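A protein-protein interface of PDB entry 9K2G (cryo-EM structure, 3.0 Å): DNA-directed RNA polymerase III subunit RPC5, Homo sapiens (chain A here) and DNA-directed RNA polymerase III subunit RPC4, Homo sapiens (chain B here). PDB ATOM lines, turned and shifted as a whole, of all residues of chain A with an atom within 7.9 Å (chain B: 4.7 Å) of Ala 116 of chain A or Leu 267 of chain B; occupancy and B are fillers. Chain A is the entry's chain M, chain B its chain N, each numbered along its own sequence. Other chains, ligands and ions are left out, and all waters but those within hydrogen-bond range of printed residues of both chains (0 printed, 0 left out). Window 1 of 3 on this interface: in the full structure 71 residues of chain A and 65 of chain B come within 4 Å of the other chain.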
ATOM      1  N   TYR A  16      23.981 -12.185  22.096  1.00  0.00           N
ATOM      2  CA  TYR A  16      25.220 -12.729  21.575  1.00  0.00           C
ATOM      3  C   TYR A  16      26.212 -11.603  21.311  1.00  0.00           C
ATOM      4  O   TYR A  16      25.839 -10.436  21.178  1.00  0.00           O
ATOM      5  CB  TYR A  16      24.976 -13.513  20.280  1.00  0.00           C
ATOM      6  CG  TYR A  16      23.988 -14.652  20.415  1.00  0.00           C
ATOM      7  CD1 TYR A  16      24.099 -15.575  21.449  1.00  0.00           C
ATOM      8  CD2 TYR A  16      22.942 -14.804  19.519  1.00  0.00           C
ATOM      9  CE1 TYR A  16      23.198 -16.615  21.577  1.00  0.00           C
ATOM     10  CE2 TYR A  16      22.038 -15.836  19.638  1.00  0.00           C
ATOM     11  CZ  TYR A  16      22.166 -16.740  20.670  1.00  0.00           C
ATOM     12  OH  TYR A  16      21.266 -17.774  20.790  1.00  0.00           O
ATOM     13  N   ALA A  18      29.679 -10.579  18.844  1.00  0.00           N
ATOM     14  CA  ALA A  18      30.450 -10.884  17.642  1.00  0.00           C
ATOM     15  C   ALA A  18      31.624  -9.926  17.533  1.00  0.00           C
ATOM     16  O   ALA A  18      31.447  -8.706  17.628  1.00  0.00           O
ATOM     17  CB  ALA A  18      29.576 -10.798  16.389  1.00  0.00           C
ATOM     18  N   LEU A  25      33.975  -1.516  12.138  1.00  0.00           N
ATOM     19  CA  LEU A  25      32.617  -1.005  12.244  1.00  0.00           C
ATOM     20  C   LEU A  25      32.646   0.467  12.643  1.00  0.00           C
ATOM     21  O   LEU A  25      33.140   0.812  13.721  1.00  0.00           O
ATOM     22  CB  LEU A  25      31.807  -1.817  13.251  1.00  0.00           C
ATOM     23  CG  LEU A  25      30.291  -1.758  13.053  1.00  0.00           C
ATOM     24  CD1 LEU A  25      29.946  -2.168  11.634  1.00  0.00           C
ATOM     25  CD2 LEU A  25      29.574  -2.641  14.056  1.00  0.00           C
ATOM     26  N   TYR A  26      32.112   1.322  11.775  1.00  0.00           N
ATOM     27  CA  TYR A  26      31.965   2.746  12.044  1.00  0.00           C
ATOM     28  C   TYR A  26      30.492   3.120  11.987  1.00  0.00           C
ATOM     29  O   TYR A  26      29.697   2.488  11.286  1.00  0.00           O
ATOM     30  CB  TYR A  26      32.744   3.601  11.034  1.00  0.00           C
ATOM     31  CG  TYR A  26      34.249   3.546  11.169  1.00  0.00           C
ATOM     32  CD1 TYR A  26      34.845   3.028  12.311  1.00  0.00           C
ATOM     33  CD2 TYR A  26      35.076   4.023  10.159  1.00  0.00           C
ATOM     34  CE1 TYR A  26      36.222   2.980  12.439  1.00  0.00           C
ATOM     35  CE2 TYR A  26      36.449   3.980  10.280  1.00  0.00           C
ATOM     36  CZ  TYR A  26      37.019   3.457  11.422  1.00  0.00           C
ATOM     37  OH  TYR A  26      38.388   3.412  11.545  1.00  0.00           O
ATOM     38  N   LEU A  27      30.130   4.161  12.735  1.00  0.00           N
ATOM     39  CA  LEU A  27      28.781   4.711  12.708  1.00  0.00           C
ATOM     40  C   LEU A  27      28.837   6.100  12.095  1.00  0.00           C
ATOM     41  O   LEU A  27      29.532   6.986  12.613  1.00  0.00           O
ATOM     42  CB  LEU A  27      28.179   4.765  14.111  1.00  0.00           C
ATOM     43  CG  LEU A  27      26.758   5.334  14.200  1.00  0.00           C
ATOM     44  CD1 LEU A  27      25.791   4.504  13.371  1.00  0.00           C
ATOM     45  CD2 LEU A  27      26.302   5.411  15.651  1.00  0.00           C
ATOM     46  N   THR A 111      35.245   4.768  22.059  1.00  0.00           N
ATOM     47  CA  THR A 111      33.926   4.256  21.696  1.00  0.00           C
ATOM     48  C   THR A 111      33.689   2.859  22.266  1.00  0.00           C
ATOM     49  O   THR A 111      32.841   2.123  21.750  1.00  0.00           O
ATOM     50  CB  THR A 111      33.758   4.242  20.176  1.00  0.00           C
ATOM     51  OG1 THR A 111      34.727   3.366  19.589  1.00  0.00           O
ATOM     52  CG2 THR A 111      33.941   5.645  19.610  1.00  0.00           C
ATOM     53  N   ARG A 113      32.296   1.948  25.007  1.00  0.00           N
ATOM     54  CA  ARG A 113      31.014   1.801  25.686  1.00  0.00           C
ATOM     55  C   ARG A 113      29.828   1.768  24.726  1.00  0.00           C
ATOM     56  O   ARG A 113      28.698   1.558  25.173  1.00  0.00           O
ATOM     57  CB  ARG A 113      30.821   2.928  26.698  1.00  0.00           C
ATOM     58  CG  ARG A 113      30.864   4.322  26.104  1.00  0.00           C
ATOM     59  CD  ARG A 113      30.629   5.355  27.189  1.00  0.00           C
ATOM     60  NE  ARG A 113      29.413   5.069  27.939  1.00  0.00           N
ATOM     61  CZ  ARG A 113      29.139   5.557  29.140  1.00  0.00           C
ATOM     62  NH1 ARG A 113      29.980   6.352  29.774  1.00  0.00           N
ATOM     63  NH2 ARG A 113      27.990   5.221  29.731  1.00  0.00           N
ATOM     64  N   TYR A 114      30.052   1.980  23.430  1.00  0.00           N
ATOM     65  CA  TYR A 114      28.996   1.939  22.437  1.00  0.00           C
ATOM     66  C   TYR A 114      29.055   0.629  21.663  1.00  0.00           C
ATOM     67  O   TYR A 114      30.135   0.106  21.371  1.00  0.00           O
ATOM     68  CB  TYR A 114      29.101   3.122  21.472  1.00  0.00           C
ATOM     69  CG  TYR A 114      29.137   4.469  22.161  1.00  0.00           C
ATOM     70  CD1 TYR A 114      27.981   5.041  22.674  1.00  0.00           C
ATOM     71  CD2 TYR A 114      30.329   5.166  22.296  1.00  0.00           C
ATOM     72  CE1 TYR A 114      28.009   6.265  23.305  1.00  0.00           C
ATOM     73  CE2 TYR A 114      30.370   6.393  22.928  1.00  0.00           C
ATOM     74  CZ  TYR A 114      29.209   6.940  23.428  1.00  0.00           C
ATOM     75  OH  TYR A 114      29.247   8.166  24.055  1.00  0.00           O
ATOM     76  N   ALA A 115      27.881   0.099  21.329  1.00  0.00           N
ATOM     77  CA  ALA A 115      27.791  -1.166  20.614  1.00  0.00           C
ATOM     78  C   ALA A 115      26.620  -1.119  19.647  1.00  0.00           C
ATOM     79  O   ALA A 115      25.575  -0.537  19.947  1.00  0.00           O
ATOM     80  CB  ALA A 115      27.625  -2.339  21.584  1.00  0.00           C
ATOM     81  N   ALA A 116      26.807  -1.737  18.482  1.00  0.00           N
ATOM     82  CA  ALA A 116      25.756  -1.856  17.486  1.00  0.00           C
ATOM     83  C   ALA A 116      25.029  -3.179  17.695  1.00  0.00           C
ATOM     84  O   ALA A 116      25.665  -4.231  17.816  1.00  0.00           O
ATOM     85  CB  ALA A 116      26.331  -1.781  16.069  1.00  0.00           C
ATOM     86  N   ALA A 117      23.702  -3.117  17.740  1.00  0.00           N
ATOM     87  CA  ALA A 117      22.864  -4.267  18.055  1.00  0.00           C
ATOM     88  C   ALA A 117      22.027  -4.622  16.826  1.00  0.00           C
ATOM     89  O   ALA A 117      21.163  -3.847  16.410  1.00  0.00           O
ATOM     90  CB  ALA A 117      21.968  -3.974  19.255  1.00  0.00           C
ATOM     91  N   LEU A 118      22.296  -5.790  16.257  1.00  0.00           N
ATOM     92  CA  LEU A 118      21.462  -6.343  15.199  1.00  0.00           C
ATOM     93  C   LEU A 118      20.451  -7.290  15.832  1.00  0.00           C
ATOM     94  O   LEU A 118      20.830  -8.211  16.564  1.00  0.00           O
ATOM     95  CB  LEU A 118      22.309  -7.068  14.152  1.00  0.00           C
ATOM     96  CG  LEU A 118      21.635  -7.458  12.828  1.00  0.00           C
ATOM     97  CD1 LEU A 118      22.650  -7.476  11.700  1.00  0.00           C
ATOM     98  CD2 LEU A 118      20.953  -8.810  12.929  1.00  0.00           C
ATOM     99  N   TYR A 119      19.173  -7.064  15.552  1.00  0.00           N
ATOM    100  CA  TYR A 119      18.101  -7.817  16.178  1.00  0.00           C
ATOM    101  C   TYR A 119      17.515  -8.818  15.190  1.00  0.00           C
ATOM    102  O   TYR A 119      17.168  -8.452  14.063  1.00  0.00           O
ATOM    103  CB  TYR A 119      17.005  -6.884  16.692  1.00  0.00           C
ATOM    104  CG  TYR A 119      15.836  -7.611  17.319  1.00  0.00           C
ATOM    105  CD1 TYR A 119      16.014  -8.394  18.453  1.00  0.00           C
ATOM    106  CD2 TYR A 119      14.557  -7.512  16.785  1.00  0.00           C
ATOM    107  CE1 TYR A 119      14.953  -9.062  19.034  1.00  0.00           C
ATOM    108  CE2 TYR A 119      13.488  -8.176  17.361  1.00  0.00           C
ATOM    109  CZ  TYR A 119      13.695  -8.946  18.483  1.00  0.00           C
ATOM    110  OH  TYR A 119      12.639  -9.611  19.061  1.00  0.00           O
ATOM    111  N   LEU A 124      19.730 -10.957  19.968  1.00  0.00           N
ATOM    112  CA  LEU A 124      20.309  -9.637  19.767  1.00  0.00           C
ATOM    113  C   LEU A 124      21.824  -9.767  19.756  1.00  0.00           C
ATOM    114  O   LEU A 124      22.419 -10.172  20.759  1.00  0.00           O
ATOM    115  CB  LEU A 124      19.861  -8.663  20.862  1.00  0.00           C
ATOM    116  CG  LEU A 124      20.199  -7.186  20.663  1.00  0.00           C
ATOM    117  CD1 LEU A 124      19.490  -6.647  19.438  1.00  0.00           C
ATOM    118  CD2 LEU A 124      19.830  -6.384  21.904  1.00  0.00           C
ATOM    119  N   HIS A 125      22.447  -9.431  18.628  1.00  0.00           N
ATOM    120  CA  HIS A 125      23.892  -9.557  18.455  1.00  0.00           C
ATOM    121  C   HIS A 125      24.536  -8.187  18.622  1.00  0.00           C
ATOM    122  O   HIS A 125      24.161  -7.236  17.931  1.00  0.00           O
ATOM    123  CB  HIS A 125      24.225 -10.140  17.081  1.00  0.00           C
ATOM    124  CG  HIS A 125      23.673 -11.511  16.852  1.00  0.00           C
ATOM    125  ND1 HIS A 125      24.476 -12.615  16.668  1.00  0.00           N
ATOM    126  CD2 HIS A 125      22.398 -11.957  16.767  1.00  0.00           C
ATOM    127  CE1 HIS A 125      23.719 -13.681  16.480  1.00  0.00           C
ATOM    128  NE2 HIS A 125      22.455 -13.312  16.539  1.00  0.00           N
ATOM    129  N   LEU A 126      25.499  -8.092  19.529  1.00  0.00           N
ATOM    130  CA  LEU A 126      26.204  -6.847  19.803  1.00  0.00           C
ATOM    131  C   LEU A 126      27.595  -6.885  19.185  1.00  0.00           C
ATOM    132  O   LEU A 126      28.276  -7.912  19.193  1.00  0.00           O
ATOM    133  CB  LEU A 126      26.316  -6.603  21.308  1.00  0.00           C
ATOM    134  CG  LEU A 126      25.066  -6.825  22.167  1.00  0.00           C
ATOM    135  CD1 LEU A 126      25.304  -6.336  23.591  1.00  0.00           C
ATOM    136  CD2 LEU A 126      23.845  -6.153  21.559  1.00  0.00           C
ATOM    137  N   THR A 127      28.016  -5.737  18.648  1.00  0.00           N
ATOM    138  CA  THR A 127      29.343  -5.606  18.064  1.00  0.00           C
ATOM    139  C   THR A 127      29.945  -4.267  18.489  1.00  0.00           C
ATOM    140  O   THR A 127      29.285  -3.221  18.347  1.00  0.00           O
ATOM    141  CB  THR A 127      29.301  -5.710  16.538  1.00  0.00           C
ATOM    142  OG1 THR A 127      28.736  -6.973  16.161  1.00  0.00           O
ATOM    143  CG2 THR A 127      30.702  -5.601  15.953  1.00  0.00           C
ATOM    144  N   PRO A 128      31.170  -4.264  19.016  1.00  0.00           N
ATOM    145  CA  PRO A 128      31.796  -2.994  19.402  1.00  0.00           C
ATOM    146  C   PRO A 128      32.054  -2.109  18.192  1.00  0.00           C
ATOM    147  O   PRO A 128      32.263  -2.585  17.076  1.00  0.00           O
ATOM    148  CB  PRO A 128      33.110  -3.430  20.063  1.00  0.00           C
ATOM    149  CG  PRO A 128      32.887  -4.863  20.453  1.00  0.00           C
ATOM    150  CD  PRO A 128      31.989  -5.425  19.401  1.00  0.00           C
ATOM    151  N   LEU A 129      32.037  -0.798  18.430  1.00  0.00           N
ATOM    152  CA  LEU A 129      32.272   0.196  17.391  1.00  0.00           C
ATOM    153  C   LEU A 129      33.701   0.705  17.479  1.00  0.00           C
ATOM    154  O   LEU A 129      34.155   1.133  18.545  1.00  0.00           O
ATOM    155  CB  LEU A 129      31.298   1.370  17.513  1.00  0.00           C
ATOM    156  CG  LEU A 129      29.962   1.245  16.776  1.00  0.00           C
ATOM    157  CD1 LEU A 129      29.134   0.108  17.335  1.00  0.00           C
ATOM    158  CD2 LEU A 129      29.192   2.555  16.829  1.00  0.00           C
ATOM    159  N   LEU A 225      27.853  -9.606  11.307  1.00  0.00           N
ATOM    160  CA  LEU A 225      27.445  -9.100  12.610  1.00  0.00           C
ATOM    161  C   LEU A 225      26.946 -10.204  13.529  1.00  0.00           C
ATOM    162  O   LEU A 225      26.818  -9.976  14.737  1.00  0.00           O
ATOM    163  CB  LEU A 225      26.368  -8.025  12.452  1.00  0.00           C
ATOM    164  CG  LEU A 225      26.840  -6.672  11.908  1.00  0.00           C
ATOM    165  CD1 LEU A 225      25.732  -5.637  12.011  1.00  0.00           C
ATOM    166  CD2 LEU A 225      28.081  -6.206  12.647  1.00  0.00           C
ATOM    167  N   LEU B 254       9.996  -3.741  21.548  1.00  0.00           N
ATOM    168  CA  LEU B 254      10.333  -5.125  21.221  1.00  0.00           C
ATOM    169  C   LEU B 254       9.088  -5.953  20.926  1.00  0.00           C
ATOM    170  O   LEU B 254       9.106  -6.836  20.062  1.00  0.00           O
ATOM    171  CB  LEU B 254      11.144  -5.751  22.359  1.00  0.00           C
ATOM    172  CG  LEU B 254      12.485  -5.081  22.667  1.00  0.00           C
ATOM    173  CD1 LEU B 254      13.226  -5.835  23.763  1.00  0.00           C
ATOM    174  CD2 LEU B 254      13.345  -4.975  21.415  1.00  0.00           C
ATOM    175  N   GLU B 257       8.172  -5.255  17.559  1.00  0.00           N
ATOM    176  CA  GLU B 257       9.256  -5.702  16.691  1.00  0.00           C
ATOM    177  C   GLU B 257       9.209  -7.204  16.447  1.00  0.00           C
ATOM    178  O   GLU B 257       9.699  -7.679  15.417  1.00  0.00           O
ATOM    179  CB  GLU B 257      10.610  -5.312  17.289  1.00  0.00           C
ATOM    180  CG  GLU B 257      11.041  -3.882  17.013  1.00  0.00           C
ATOM    181  CD  GLU B 257      12.419  -3.578  17.562  1.00  0.00           C
ATOM    182  OE1 GLU B 257      13.009  -4.477  18.197  1.00  0.00           O
ATOM    183  OE2 GLU B 257      12.913  -2.452  17.364  1.00  0.00           O
ATOM    184  N   GLU B 265      15.771  -5.706  12.705  1.00  0.00           N
ATOM    185  CA  GLU B 265      15.996  -4.294  12.986  1.00  0.00           C
ATOM    186  C   GLU B 265      17.409  -4.093  13.504  1.00  0.00           C
ATOM    187  O   GLU B 265      17.970  -4.966  14.172  1.00  0.00           O
ATOM    188  CB  GLU B 265      14.968  -3.759  14.000  1.00  0.00           C
ATOM    189  CG  GLU B 265      15.112  -2.282  14.333  1.00  0.00           C
ATOM    190  CD  GLU B 265      14.979  -1.389  13.112  1.00  0.00           C
ATOM    191  OE1 GLU B 265      14.155  -1.707  12.227  1.00  0.00           O
ATOM    192  OE2 GLU B 265      15.702  -0.375  13.034  1.00  0.00           O
ATOM    193  N   LEU B 266      17.982  -2.936  13.184  1.00  0.00           N
ATOM    194  CA  LEU B 266      19.301  -2.541  13.665  1.00  0.00           C
ATOM    195  C   LEU B 266      19.128  -1.573  14.828  1.00  0.00           C
ATOM    196  O   LEU B 266      18.501  -0.518  14.673  1.00  0.00           O
ATOM    197  CB  LEU B 266      20.129  -1.906  12.552  1.00  0.00           C
ATOM    198  CG  LEU B 266      21.001  -2.828  11.699  1.00  0.00           C
ATOM    199  CD1 LEU B 266      22.027  -3.552  12.560  1.00  0.00           C
ATOM    200  CD2 LEU B 266      20.153  -3.817  10.913  1.00  0.00           C
ATOM    201  N   LEU B 267      19.685  -1.924  15.982  1.00  0.00           N
ATOM    202  CA  LEU B 267      19.603  -1.103  17.180  1.00  0.00           C
ATOM    203  C   LEU B 267      20.984  -0.603  17.576  1.00  0.00           C
ATOM    204  O   LEU B 267      22.015  -1.178  17.212  1.00  0.00           O
ATOM    205  CB  LEU B 267      18.973  -1.881  18.341  1.00  0.00           C
ATOM    206  CG  LEU B 267      17.470  -2.138  18.249  1.00  0.00           C
ATOM    207  CD1 LEU B 267      16.960  -2.803  19.521  1.00  0.00           C
ATOM    208  CD2 LEU B 267      16.720  -0.841  17.974  1.00  0.00           C
ATOM    209  N   PHE B 268      20.995   0.495  18.335  1.00  0.00           N
ATOM    210  CA  PHE B 268      22.219   1.138  18.799  1.00  0.00           C
ATOM    211  C   PHE B 268      22.086   1.349  20.305  1.00  0.00           C
ATOM    212  O   PHE B 268      21.458   2.314  20.751  1.00  0.00           O
ATOM    213  CB  PHE B 268      22.452   2.454  18.061  1.00  0.00           C
ATOM    214  CG  PHE B 268      23.596   3.264  18.608  1.00  0.00           C
ATOM    215  CD1 PHE B 268      24.907   2.912  18.335  1.00  0.00           C
ATOM    216  CD2 PHE B 268      23.354   4.387  19.380  1.00  0.00           C
ATOM    217  CE1 PHE B 268      25.957   3.664  18.832  1.00  0.00           C
ATOM    218  CE2 PHE B 268      24.398   5.138  19.880  1.00  0.00           C
ATOM    219  CZ  PHE B 268      25.703   4.776  19.605  1.00  0.00           C
ATOM    220  N   LEU B 269      22.672   0.452  21.089  1.00  0.00           N
ATOM    221  CA  LEU B 269      22.579   0.505  22.543  1.00  0.00           C
ATOM    222  C   LEU B 269      23.895   0.977  23.141  1.00  0.00           C
ATOM    223  O   LEU B 269      24.974   0.593  22.679  1.00  0.00           O
ATOM    224  CB  LEU B 269      22.182  -0.858  23.124  1.00  0.00           C
ATOM    225  CG  LEU B 269      22.965  -2.126  22.785  1.00  0.00           C
ATOM    226  CD1 LEU B 269      24.163  -2.326  23.711  1.00  0.00           C
ATOM    227  CD2 LEU B 269      22.036  -3.324  22.854  1.00  0.00           C
ATOM    228  N   LEU B 360      24.590   2.640   9.737  1.00  0.00           N
ATOM    229  CA  LEU B 360      25.594   1.706  10.237  1.00  0.00           C
ATOM    230  C   LEU B 360      26.295   1.072   9.042  1.00  0.00           C
ATOM    231  O   LEU B 360      25.669   0.362   8.249  1.00  0.00           O
ATOM    232  CB  LEU B 360      24.952   0.640  11.118  1.00  0.00           C
ATOM    233  CG  LEU B 360      25.860  -0.491  11.596  1.00  0.00           C
ATOM    234  CD1 LEU B 360      27.088   0.064  12.286  1.00  0.00           C
ATOM    235  CD2 LEU B 360      25.100  -1.425  12.522  1.00  0.00           C
ATOM    236  N   HIS B 381      16.492   3.571  16.358  1.00  0.00           N
ATOM    237  CA  HIS B 381      16.260   3.744  17.786  1.00  0.00           C
ATOM    238  C   HIS B 381      17.537   3.491  18.566  1.00  0.00           C
ATOM    239  O   HIS B 381      18.398   2.712  18.147  1.00  0.00           O
ATOM    240  CB  HIS B 381      15.150   2.802  18.280  1.00  0.00           C
ATOM    241  CG  HIS B 381      13.934   2.799  17.410  1.00  0.00           C
ATOM    242  ND1 HIS B 381      13.571   1.708  16.645  1.00  0.00           N
ATOM    243  CD2 HIS B 381      13.003   3.753  17.173  1.00  0.00           C
ATOM    244  CE1 HIS B 381      12.469   1.990  15.977  1.00  0.00           C
ATOM    245  NE2 HIS B 381      12.099   3.223  16.280  1.00  0.00           N
ATOM    246  N   LEU B 383      19.163   2.585  22.461  1.00  0.00           N
ATOM    247  CA  LEU B 383      18.934   2.032  23.787  1.00  0.00           C
ATOM    248  C   LEU B 383      20.028   2.495  24.737  1.00  0.00           C
ATOM    249  O   LEU B 383      21.167   2.741  24.328  1.00  0.00           O
ATOM    250  CB  LEU B 383      18.897   0.500  23.749  1.00  0.00           C
ATOM    251  CG  LEU B 383      17.875  -0.160  22.823  1.00  0.00           C
ATOM    252  CD1 LEU B 383      17.911  -1.675  22.978  1.00  0.00           C
ATOM    253  CD2 LEU B 383      16.474   0.378  23.095  1.00  0.00           C
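Leu 360 of chain B touches Leu 25 of chain A (CD1 to CD1, 3.7 Å).
Leu 360 of chain B touches Tyr 26 of chain A.
Phe 268 of chain B touches Leu 27 of chain A.
Tyr 114 of chain A touches Phe 268 of chain B (CD1 to CZ, 3.8 Å).
Ala 115 of chain A touches Phe 268 of chain B (O to CD1, 3.9 Å).
Ala 117 of chain A touches Leu 269 of chain B (CB to CD2, 3.7 Å).
CB of Leu 118 of chain A touches CD1 of Leu 266 of chain B, at 3.9 Å.
CD2 of Tyr 119 of chain A touches OE1 of Glu 257 of chain B (3.7 Å).
CD2 of Leu 269 of chain B touches CD2 of Leu 124 of chain A (3.9 Å).
Leu 126 of chain A touches Leu 269 of chain B (CD2 to CD2, 3.6 Å).
N of Tyr 16 of chain A lies within hydrogen-bond range of O of Leu 124 of chain A (2.9 Å).
The backbone carbonyl oxygen (O) of Tyr 16 of chain A is in hydrogen-bond range of the backbone NH (N) of Leu 126 of chain A (2.9 Å).
The side-chain hydroxyl (OG1) of Thr 111 of chain A sits at hydrogen-bond distance from the backbone carbonyl oxygen (O) of Leu 129 of chain A (2.5 Å).
N of Ala 116 of chain A sits at hydrogen-bond distance from O of Thr 127 of chain A (2.9 Å).
N of Phe 268 of chain B lies within hydrogen-bond range of O of His 381 of chain B (3.4 Å).
The backbone carbonyl oxygen (O) of Phe 268 of chain B sits at hydrogen-bond distance from the backbone NH (N) of Leu 383 of chain B (2.9 Å).
Ala 18 of chain A touches none of the printed residues of chain B.
Of the printed residues of chain B, Leu 27 of chain A touches Phe 268 (3.6 Å).
Arg 113 of chain A touches none of the printed residues of chain B.
Ala 116 of chain A touches two residues of chain B.
Printed residues of chain B within 4 Å of Ala 117 of chain A: Leu 266, Leu 267 and Leu 269.
Of the printed residues of chain B, Tyr 119 of chain A touches Glu 257 and Glu 265.
Of the printed residues of chain B, Leu 124 of chain A touches Leu 269.
Of chain A, only Ala 116 and Ala 117 come within 4 Å of Leu 267 of chain B.
O of Leu 269 of chain B lies within hydrogen-bond range of N of Ala 115 of chain A (3.2 Å).
The backbone carbonyl oxygen (O) of Ala 117 of chain A lies within hydrogen-bond range of the backbone NH (N) of Leu 267 of chain B, 2.5 Å away.
N of Tyr 119 of chain A is in hydrogen-bond range of O of Glu 265 of chain B.
Hydrophobic or aromatic side chains of chain B that line the printed part of chain A: Leu 266, Leu 267, Phe 268, Leu 269 and Leu 360.
Along chain A the printed residues that touch a printed residue of chain B span positions 25 to 129.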
